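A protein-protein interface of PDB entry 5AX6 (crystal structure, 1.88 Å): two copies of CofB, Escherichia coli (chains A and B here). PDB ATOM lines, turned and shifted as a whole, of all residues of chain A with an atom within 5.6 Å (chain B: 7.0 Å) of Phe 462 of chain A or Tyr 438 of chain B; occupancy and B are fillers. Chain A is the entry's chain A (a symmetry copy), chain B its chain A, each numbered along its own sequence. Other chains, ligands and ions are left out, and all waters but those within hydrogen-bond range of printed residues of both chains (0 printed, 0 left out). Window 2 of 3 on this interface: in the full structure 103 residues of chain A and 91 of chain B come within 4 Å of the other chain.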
ATOM      1  N   THR A 412     -23.129   5.999  27.500  1.00  0.00           N
ATOM      2  CA  THR A 412     -24.402   5.853  28.208  1.00  0.00           C
ATOM      3  C   THR A 412     -24.600   7.061  29.119  1.00  0.00           C
ATOM      4  O   THR A 412     -23.675   7.840  29.316  1.00  0.00           O
ATOM      5  CB  THR A 412     -24.449   4.559  29.034  1.00  0.00           C
ATOM      6  OG1 THR A 412     -23.353   4.543  29.961  1.00  0.00           O
ATOM      7  CG2 THR A 412     -24.360   3.339  28.114  1.00  0.00           C
ATOM      8  N   GLY A 437     -20.887   1.450  27.711  1.00  0.00           N
ATOM      9  CA  GLY A 437     -21.565   0.164  27.749  1.00  0.00           C
ATOM     10  C   GLY A 437     -20.938  -0.771  26.732  1.00  0.00           C
ATOM     11  O   GLY A 437     -19.754  -0.622  26.401  1.00  0.00           O
ATOM     12  N   TYR A 438     -21.711  -1.737  26.239  1.00  0.00           N
ATOM     13  CA  TYR A 438     -21.215  -2.654  25.214  1.00  0.00           C
ATOM     14  C   TYR A 438     -21.732  -2.210  23.855  1.00  0.00           C
ATOM     15  O   TYR A 438     -22.907  -1.905  23.699  1.00  0.00           O
ATOM     16  CB  TYR A 438     -21.652  -4.095  25.469  1.00  0.00           C
ATOM     17  CG  TYR A 438     -21.417  -4.584  26.873  1.00  0.00           C
ATOM     18  CD1 TYR A 438     -20.411  -4.043  27.662  1.00  0.00           C
ATOM     19  CD2 TYR A 438     -22.207  -5.589  27.414  1.00  0.00           C
ATOM     20  CE1 TYR A 438     -20.198  -4.493  28.963  1.00  0.00           C
ATOM     21  CE2 TYR A 438     -22.009  -6.037  28.711  1.00  0.00           C
ATOM     22  CZ  TYR A 438     -21.004  -5.488  29.477  1.00  0.00           C
ATOM     23  OH  TYR A 438     -20.807  -5.939  30.759  1.00  0.00           O
ATOM     24  N   LEU A 439     -20.847  -2.174  22.873  1.00  0.00           N
ATOM     25  CA  LEU A 439     -21.231  -1.762  21.532  1.00  0.00           C
ATOM     26  C   LEU A 439     -21.920  -2.900  20.771  1.00  0.00           C
ATOM     27  O   LEU A 439     -21.427  -4.030  20.763  1.00  0.00           O
ATOM     28  CB  LEU A 439     -19.979  -1.299  20.783  1.00  0.00           C
ATOM     29  CG  LEU A 439     -20.085  -0.557  19.469  1.00  0.00           C
ATOM     30  CD1 LEU A 439     -20.907   0.714  19.667  1.00  0.00           C
ATOM     31  CD2 LEU A 439     -18.662  -0.251  19.000  1.00  0.00           C
ATOM     32  N   SER A 440     -23.058  -2.617  20.142  1.00  0.00           N
ATOM     33  CA  SER A 440     -23.657  -3.572  19.206  1.00  0.00           C
ATOM     34  C   SER A 440     -23.225  -3.244  17.778  1.00  0.00           C
ATOM     35  O   SER A 440     -23.304  -4.085  16.872  1.00  0.00           O
ATOM     36  CB  SER A 440     -25.176  -3.562  19.303  1.00  0.00           C
ATOM     37  OG  SER A 440     -25.596  -4.126  20.531  1.00  0.00           O
ATOM     38  N   GLY A 460     -26.379   0.746  18.202  1.00  0.00           N
ATOM     39  CA  GLY A 460     -26.916  -0.088  19.262  1.00  0.00           C
ATOM     40  C   GLY A 460     -25.948  -0.164  20.422  1.00  0.00           C
ATOM     41  O   GLY A 460     -24.758  -0.420  20.233  1.00  0.00           O
ATOM     42  N   VAL A 461     -26.458   0.062  21.632  1.00  0.00           N
ATOM     43  CA  VAL A 461     -25.641   0.040  22.838  1.00  0.00           C
ATOM     44  C   VAL A 461     -26.379  -0.675  23.971  1.00  0.00           C
ATOM     45  O   VAL A 461     -27.568  -0.446  24.181  1.00  0.00           O
ATOM     46  CB  VAL A 461     -25.266   1.475  23.280  1.00  0.00           C
ATOM     47  CG1 VAL A 461     -24.655   1.481  24.686  1.00  0.00           C
ATOM     48  CG2 VAL A 461     -24.304   2.124  22.259  1.00  0.00           C
ATOM     49  N   PHE A 462     -25.680  -1.556  24.676  1.00  0.00           N
ATOM     50  CA  PHE A 462     -26.234  -2.156  25.884  1.00  0.00           C
ATOM     51  C   PHE A 462     -25.617  -1.516  27.112  1.00  0.00           C
ATOM     52  O   PHE A 462     -24.400  -1.462  27.237  1.00  0.00           O
ATOM     53  CB  PHE A 462     -26.001  -3.667  25.919  1.00  0.00           C
ATOM     54  CG  PHE A 462     -26.512  -4.320  27.184  1.00  0.00           C
ATOM     55  CD1 PHE A 462     -27.870  -4.505  27.379  1.00  0.00           C
ATOM     56  CD2 PHE A 462     -25.634  -4.722  28.180  1.00  0.00           C
ATOM     57  CE1 PHE A 462     -28.345  -5.095  28.545  1.00  0.00           C
ATOM     58  CE2 PHE A 462     -26.100  -5.315  29.345  1.00  0.00           C
ATOM     59  CZ  PHE A 462     -27.456  -5.499  29.527  1.00  0.00           C
ATOM     60  N   ASP A 463     -26.461  -1.032  28.017  1.00  0.00           N
ATOM     61  CA  ASP A 463     -25.998  -0.431  29.260  1.00  0.00           C
ATOM     62  C   ASP A 463     -26.010  -1.490  30.362  1.00  0.00           C
ATOM     63  O   ASP A 463     -27.071  -1.861  30.851  1.00  0.00           O
ATOM     64  CB  ASP A 463     -26.884   0.762  29.644  1.00  0.00           C
ATOM     65  CG  ASP A 463     -26.336   1.553  30.830  1.00  0.00           C
ATOM     66  OD1 ASP A 463     -25.499   1.023  31.593  1.00  0.00           O
ATOM     67  OD2 ASP A 463     -26.751   2.721  30.994  1.00  0.00           O
ATOM     68  N   PRO A 464     -24.823  -1.979  30.756  1.00  0.00           N
ATOM     69  CA  PRO A 464     -24.735  -3.063  31.749  1.00  0.00           C
ATOM     70  C   PRO A 464     -25.107  -2.608  33.163  1.00  0.00           C
ATOM     71  O   PRO A 464     -25.545  -3.427  33.970  1.00  0.00           O
ATOM     72  CB  PRO A 464     -23.266  -3.493  31.674  1.00  0.00           C
ATOM     73  CG  PRO A 464     -22.544  -2.299  31.146  1.00  0.00           C
ATOM     74  CD  PRO A 464     -23.504  -1.583  30.237  1.00  0.00           C
ATOM     75  N   ASN A 467     -28.882  -2.600  32.762  1.00  0.00           N
ATOM     76  CA  ASN A 467     -29.377  -3.708  31.948  1.00  0.00           C
ATOM     77  C   ASN A 467     -30.395  -3.246  30.910  1.00  0.00           C
ATOM     78  O   ASN A 467     -31.443  -3.861  30.732  1.00  0.00           O
ATOM     79  CB  ASN A 467     -29.990  -4.792  32.836  1.00  0.00           C
ATOM     80  CG  ASN A 467     -28.999  -5.876  33.194  1.00  0.00           C
ATOM     81  OD1 ASN A 467     -27.792  -5.639  33.254  1.00  0.00           O
ATOM     82  ND2 ASN A 467     -29.503  -7.083  33.423  1.00  0.00           N
ATOM     83  N   THR A 468     -30.073  -2.160  30.219  1.00  0.00           N
ATOM     84  CA  THR A 468     -31.003  -1.545  29.281  1.00  0.00           C
ATOM     85  C   THR A 468     -30.396  -1.496  27.885  1.00  0.00           C
ATOM     86  O   THR A 468     -29.221  -1.168  27.725  1.00  0.00           O
ATOM     87  CB  THR A 468     -31.390  -0.118  29.734  1.00  0.00           C
ATOM     88  OG1 THR A 468     -31.912  -0.165  31.070  1.00  0.00           O
ATOM     89  CG2 THR A 468     -32.426   0.490  28.797  1.00  0.00           C
ATOM     90  N   THR A 469     -31.195  -1.838  26.882  1.00  0.00           N
ATOM     91  CA  THR A 469     -30.736  -1.809  25.495  1.00  0.00           C
ATOM     92  C   THR A 469     -31.203  -0.539  24.798  1.00  0.00           C
ATOM     93  O   THR A 469     -32.388  -0.188  24.838  1.00  0.00           O
ATOM     94  CB  THR A 469     -31.227  -3.044  24.725  1.00  0.00           C
ATOM     95  OG1 THR A 469     -30.733  -4.223  25.370  1.00  0.00           O
ATOM     96  CG2 THR A 469     -30.730  -3.015  23.290  1.00  0.00           C
ATOM     97  N   TYR A 470     -30.258   0.147  24.157  1.00  0.00           N
ATOM     98  CA  TYR A 470     -30.515   1.436  23.545  1.00  0.00           C
ATOM     99  C   TYR A 470     -30.232   1.421  22.054  1.00  0.00           C
ATOM    100  O   TYR A 470     -29.352   0.703  21.590  1.00  0.00           O
ATOM    101  CB  TYR A 470     -29.654   2.518  24.198  1.00  0.00           C
ATOM    102  CG  TYR A 470     -30.083   2.885  25.596  1.00  0.00           C
ATOM    103  CD1 TYR A 470     -31.161   3.738  25.809  1.00  0.00           C
ATOM    104  CD2 TYR A 470     -29.405   2.389  26.701  1.00  0.00           C
ATOM    105  CE1 TYR A 470     -31.557   4.083  27.090  1.00  0.00           C
ATOM    106  CE2 TYR A 470     -29.791   2.731  27.990  1.00  0.00           C
ATOM    107  CZ  TYR A 470     -30.868   3.574  28.176  1.00  0.00           C
ATOM    108  OH  TYR A 470     -31.253   3.915  29.450  1.00  0.00           O
ATOM    109  N   ALA B 410     -23.490  -6.319  15.272  1.00  0.00           N
ATOM    110  CA  ALA B 410     -23.419  -7.655  15.838  1.00  0.00           C
ATOM    111  C   ALA B 410     -24.747  -8.383  15.649  1.00  0.00           C
ATOM    112  O   ALA B 410     -25.470  -8.637  16.611  1.00  0.00           O
ATOM    113  CB  ALA B 410     -23.051  -7.578  17.312  1.00  0.00           C
ATOM    114  N   THR B 412     -27.562 -11.249  15.042  1.00  0.00           N
ATOM    115  CA  THR B 412     -27.738 -12.618  15.529  1.00  0.00           C
ATOM    116  C   THR B 412     -28.972 -13.224  14.864  1.00  0.00           C
ATOM    117  O   THR B 412     -29.738 -12.509  14.228  1.00  0.00           O
ATOM    118  CB  THR B 412     -27.889 -12.665  17.056  1.00  0.00           C
ATOM    119  OG1 THR B 412     -28.998 -11.844  17.452  1.00  0.00           O
ATOM    120  CG2 THR B 412     -26.612 -12.161  17.732  1.00  0.00           C
ATOM    121  N   LEU B 436     -29.591  -7.440  17.661  1.00  0.00           N
ATOM    122  CA  LEU B 436     -28.165  -7.222  17.901  1.00  0.00           C
ATOM    123  C   LEU B 436     -27.646  -7.810  19.212  1.00  0.00           C
ATOM    124  O   LEU B 436     -28.282  -7.703  20.260  1.00  0.00           O
ATOM    125  CB  LEU B 436     -27.847  -5.721  17.841  1.00  0.00           C
ATOM    126  CG  LEU B 436     -28.142  -5.023  16.502  1.00  0.00           C
ATOM    127  CD1 LEU B 436     -27.401  -3.693  16.392  1.00  0.00           C
ATOM    128  CD2 LEU B 436     -27.839  -5.912  15.287  1.00  0.00           C
ATOM    129  N   GLY B 437     -26.481  -8.445  19.133  1.00  0.00           N
ATOM    130  CA  GLY B 437     -25.776  -8.901  20.319  1.00  0.00           C
ATOM    131  C   GLY B 437     -24.691  -7.903  20.680  1.00  0.00           C
ATOM    132  O   GLY B 437     -24.815  -6.712  20.363  1.00  0.00           O
ATOM    133  N   TYR B 438     -23.636  -8.369  21.346  1.00  0.00           N
ATOM    134  CA  TYR B 438     -22.514  -7.497  21.690  1.00  0.00           C
ATOM    135  C   TYR B 438     -21.383  -7.724  20.700  1.00  0.00           C
ATOM    136  O   TYR B 438     -21.035  -8.857  20.393  1.00  0.00           O
ATOM    137  CB  TYR B 438     -21.999  -7.752  23.105  1.00  0.00           C
ATOM    138  CG  TYR B 438     -23.068  -7.799  24.164  1.00  0.00           C
ATOM    139  CD1 TYR B 438     -24.266  -7.116  24.004  1.00  0.00           C
ATOM    140  CD2 TYR B 438     -22.879  -8.530  25.329  1.00  0.00           C
ATOM    141  CE1 TYR B 438     -25.257  -7.165  24.982  1.00  0.00           C
ATOM    142  CE2 TYR B 438     -23.862  -8.591  26.305  1.00  0.00           C
ATOM    143  CZ  TYR B 438     -25.045  -7.907  26.126  1.00  0.00           C
ATOM    144  OH  TYR B 438     -26.014  -7.965  27.098  1.00  0.00           O
ATOM    145  N   LEU B 439     -20.813  -6.640  20.201  1.00  0.00           N
ATOM    146  CA  LEU B 439     -19.722  -6.741  19.244  1.00  0.00           C
ATOM    147  C   LEU B 439     -18.388  -7.032  19.941  1.00  0.00           C
ATOM    148  O   LEU B 439     -18.050  -6.383  20.932  1.00  0.00           O
ATOM    149  CB  LEU B 439     -19.639  -5.431  18.456  1.00  0.00           C
ATOM    150  CG  LEU B 439     -18.790  -5.323  17.208  1.00  0.00           C
ATOM    151  CD1 LEU B 439     -19.257  -6.357  16.187  1.00  0.00           C
ATOM    152  CD2 LEU B 439     -18.931  -3.894  16.681  1.00  0.00           C
ATOM    153  N   SER B 440     -17.635  -8.010  19.440  1.00  0.00           N
ATOM    154  CA  SER B 440     -16.255  -8.200  19.892  1.00  0.00           C
ATOM    155  C   SER B 440     -15.292  -7.485  18.947  1.00  0.00           C
ATOM    156  O   SER B 440     -14.137  -7.204  19.294  1.00  0.00           O
ATOM    157  CB  SER B 440     -15.900  -9.679  19.973  1.00  0.00           C
ATOM    158  OG  SER B 440     -16.595 -10.296  21.040  1.00  0.00           O
ATOM    159  N   GLY B 441     -15.775  -7.214  17.739  1.00  0.00           N
ATOM    160  CA  GLY B 441     -14.982  -6.510  16.747  1.00  0.00           C
ATOM    161  C   GLY B 441     -14.820  -7.284  15.458  1.00  0.00           C
ATOM    162  O   GLY B 441     -15.535  -8.247  15.209  1.00  0.00           O
ATOM    163  N   GLY B 460     -16.416 -11.231  15.667  1.00  0.00           N
ATOM    164  CA  GLY B 460     -16.819 -11.876  16.904  1.00  0.00           C
ATOM    165  C   GLY B 460     -18.066 -11.226  17.463  1.00  0.00           C
ATOM    166  O   GLY B 460     -18.143 -10.001  17.570  1.00  0.00           O
ATOM    167  N   VAL B 461     -19.052 -12.049  17.818  1.00  0.00           N
ATOM    168  CA  VAL B 461     -20.317 -11.562  18.353  1.00  0.00           C
ATOM    169  C   VAL B 461     -20.774 -12.437  19.523  1.00  0.00           C
ATOM    170  O   VAL B 461     -20.705 -13.661  19.448  1.00  0.00           O
ATOM    171  CB  VAL B 461     -21.411 -11.538  17.258  1.00  0.00           C
ATOM    172  CG1 VAL B 461     -22.798 -11.304  17.864  1.00  0.00           C
ATOM    173  CG2 VAL B 461     -21.087 -10.468  16.191  1.00  0.00           C
ATOM    174  N   PHE B 462     -21.213 -11.805  20.604  1.00  0.00           N
ATOM    175  CA  PHE B 462     -21.836 -12.539  21.699  1.00  0.00           C
ATOM    176  C   PHE B 462     -23.341 -12.354  21.658  1.00  0.00           C
ATOM    177  O   PHE B 462     -23.826 -11.230  21.629  1.00  0.00           O
ATOM    178  CB  PHE B 462     -21.299 -12.089  23.057  1.00  0.00           C
ATOM    179  CG  PHE B 462     -21.962 -12.788  24.223  1.00  0.00           C
ATOM    180  CD1 PHE B 462     -21.655 -14.106  24.517  1.00  0.00           C
ATOM    181  CD2 PHE B 462     -22.903 -12.132  25.001  1.00  0.00           C
ATOM    182  CE1 PHE B 462     -22.270 -14.756  25.581  1.00  0.00           C
ATOM    183  CE2 PHE B 462     -23.518 -12.773  26.068  1.00  0.00           C
ATOM    184  CZ  PHE B 462     -23.202 -14.086  26.354  1.00  0.00           C
ATOM    185  N   ASP B 463     -24.075 -13.461  21.657  1.00  0.00           N
ATOM    186  CA  ASP B 463     -25.531 -13.421  21.663  1.00  0.00           C
ATOM    187  C   ASP B 463     -26.028 -13.538  23.104  1.00  0.00           C
ATOM    188  O   ASP B 463     -25.983 -14.616  23.687  1.00  0.00           O
ATOM    189  CB  ASP B 463     -26.106 -14.549  20.796  1.00  0.00           C
ATOM    190  CG  ASP B 463     -27.616 -14.444  20.604  1.00  0.00           C
ATOM    191  OD1 ASP B 463     -28.293 -13.749  21.394  1.00  0.00           O
ATOM    192  OD2 ASP B 463     -28.129 -15.064  19.647  1.00  0.00           O
ATOM    193  N   PRO B 464     -26.507 -12.425  23.681  1.00  0.00           N
ATOM    194  CA  PRO B 464     -26.929 -12.417  25.091  1.00  0.00           C
ATOM    195  C   PRO B 464     -28.227 -13.194  25.330  1.00  0.00           C
ATOM    196  O   PRO B 464     -28.448 -13.684  26.437  1.00  0.00           O
ATOM    197  CB  PRO B 464     -27.112 -10.927  25.398  1.00  0.00           C
ATOM    198  CG  PRO B 464     -27.372 -10.292  24.072  1.00  0.00           C
ATOM    199  CD  PRO B 464     -26.612 -11.097  23.054  1.00  0.00           C
ATOM    200  N   LEU B 465     -29.055 -13.312  24.298  1.00  0.00           N
ATOM    201  CA  LEU B 465     -30.310 -14.055  24.384  1.00  0.00           C
ATOM    202  C   LEU B 465     -30.082 -15.544  24.643  1.00  0.00           C
ATOM    203  O   LEU B 465     -30.827 -16.172  25.395  1.00  0.00           O
ATOM    204  CB  LEU B 465     -31.127 -13.874  23.100  1.00  0.00           C
ATOM    205  CG  LEU B 465     -32.294 -12.887  23.179  1.00  0.00           C
ATOM    206  CD1 LEU B 465     -31.898 -11.641  23.959  1.00  0.00           C
ATOM    207  CD2 LEU B 465     -32.785 -12.521  21.787  1.00  0.00           C
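The backbone NH (N) of Ala 410 of chain B sits at hydrogen-bond distance from the backbone carbonyl oxygen (O) of Ser 440 of chain A (2.8 Å).
O of Gly 437 of chain B lies within hydrogen-bond range of OG of Ser 440 of chain A, 2.7 Å away.
N of Leu 439 of chain B is in hydrogen-bond range of O of Leu 439 of chain A (2.7 Å).
The backbone NH (N) of Gly 437 of chain B lies within hydrogen-bond range of the backbone carbonyl oxygen (O) of Ala 410 of chain B, 2.7 Å away.
N of Tyr 438 of chain B lies within hydrogen-bond range of O of Phe 462 of chain B, at 2.9 Å.
O of Phe 462 of chain A lies within hydrogen-bond range of N of Tyr 438 of chain A (2.9 Å).
The backbone carbonyl oxygen of Gly 460 of chain A lies within hydrogen-bond range of the backbone NH of Ser 440 of chain A (2.8 Å).
Tyr 438 of chain A touches Tyr 438 of chain B.
O of Leu 439 of chain A touches C of Tyr 438 of chain B (3.7 Å).
Ser 440 of chain A touches Leu 436 of chain B (CB to CD1, 3.7 Å).
Tyr 438 of chain B touches Phe 462 of chain A (OH to CD2, 3.4 Å).
Phe 462 of chain A touches just one residue of chain B: Tyr 438.
Of chain A, only Tyr 438 (3.6 Å), Leu 439 (3.7 Å) and Phe 462 (3.4 Å) come within 4 Å of Tyr 438 of chain B.
Of the printed residues of chain B, Tyr 438 of chain A touches Tyr 438 (3.6 Å).
Printed residues of chain B within 4 Å of Ser 440 of chain A: Ala 410, Leu 436 and Gly 437.
The nearest printed residue of chain A that does not touch Leu 436 of chain B is Gly 460 of chain A (4.6 Å).
Hydrophobic or aromatic side chains of chain B that line the printed part of chain A: Ala 410, Leu 436, Tyr 438 and Leu 439.
Of the 14 printed residues of chain A, 4 touch a printed residue of chain B.
Hydrophobic or aromatic side chains of chain A within 4 Å of the printed part of chain B: Tyr 438 and Phe 462.
Among the printed residues, 7 pairs touch across the chains.
Tyr 438 of chain B touches its own counterpart, Tyr 438 of chain A.
Leu 439 of chain A touches Tyr 438 of chain B, but with the chains exchanged Tyr 438 of chain A does not touch Leu 439 of chain B (5.8 Å).
Ser 440 of chain A touches Gly 437 of chain B, but with the chains exchanged Gly 437 of chain A does not touch Ser 440 of chain B (10.4 Å).
Phe 462 of chain A touches Tyr 438 of chain B, but with the chains exchanged Tyr 438 of chain A does not touch Phe 462 of chain B (7.0 Å).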
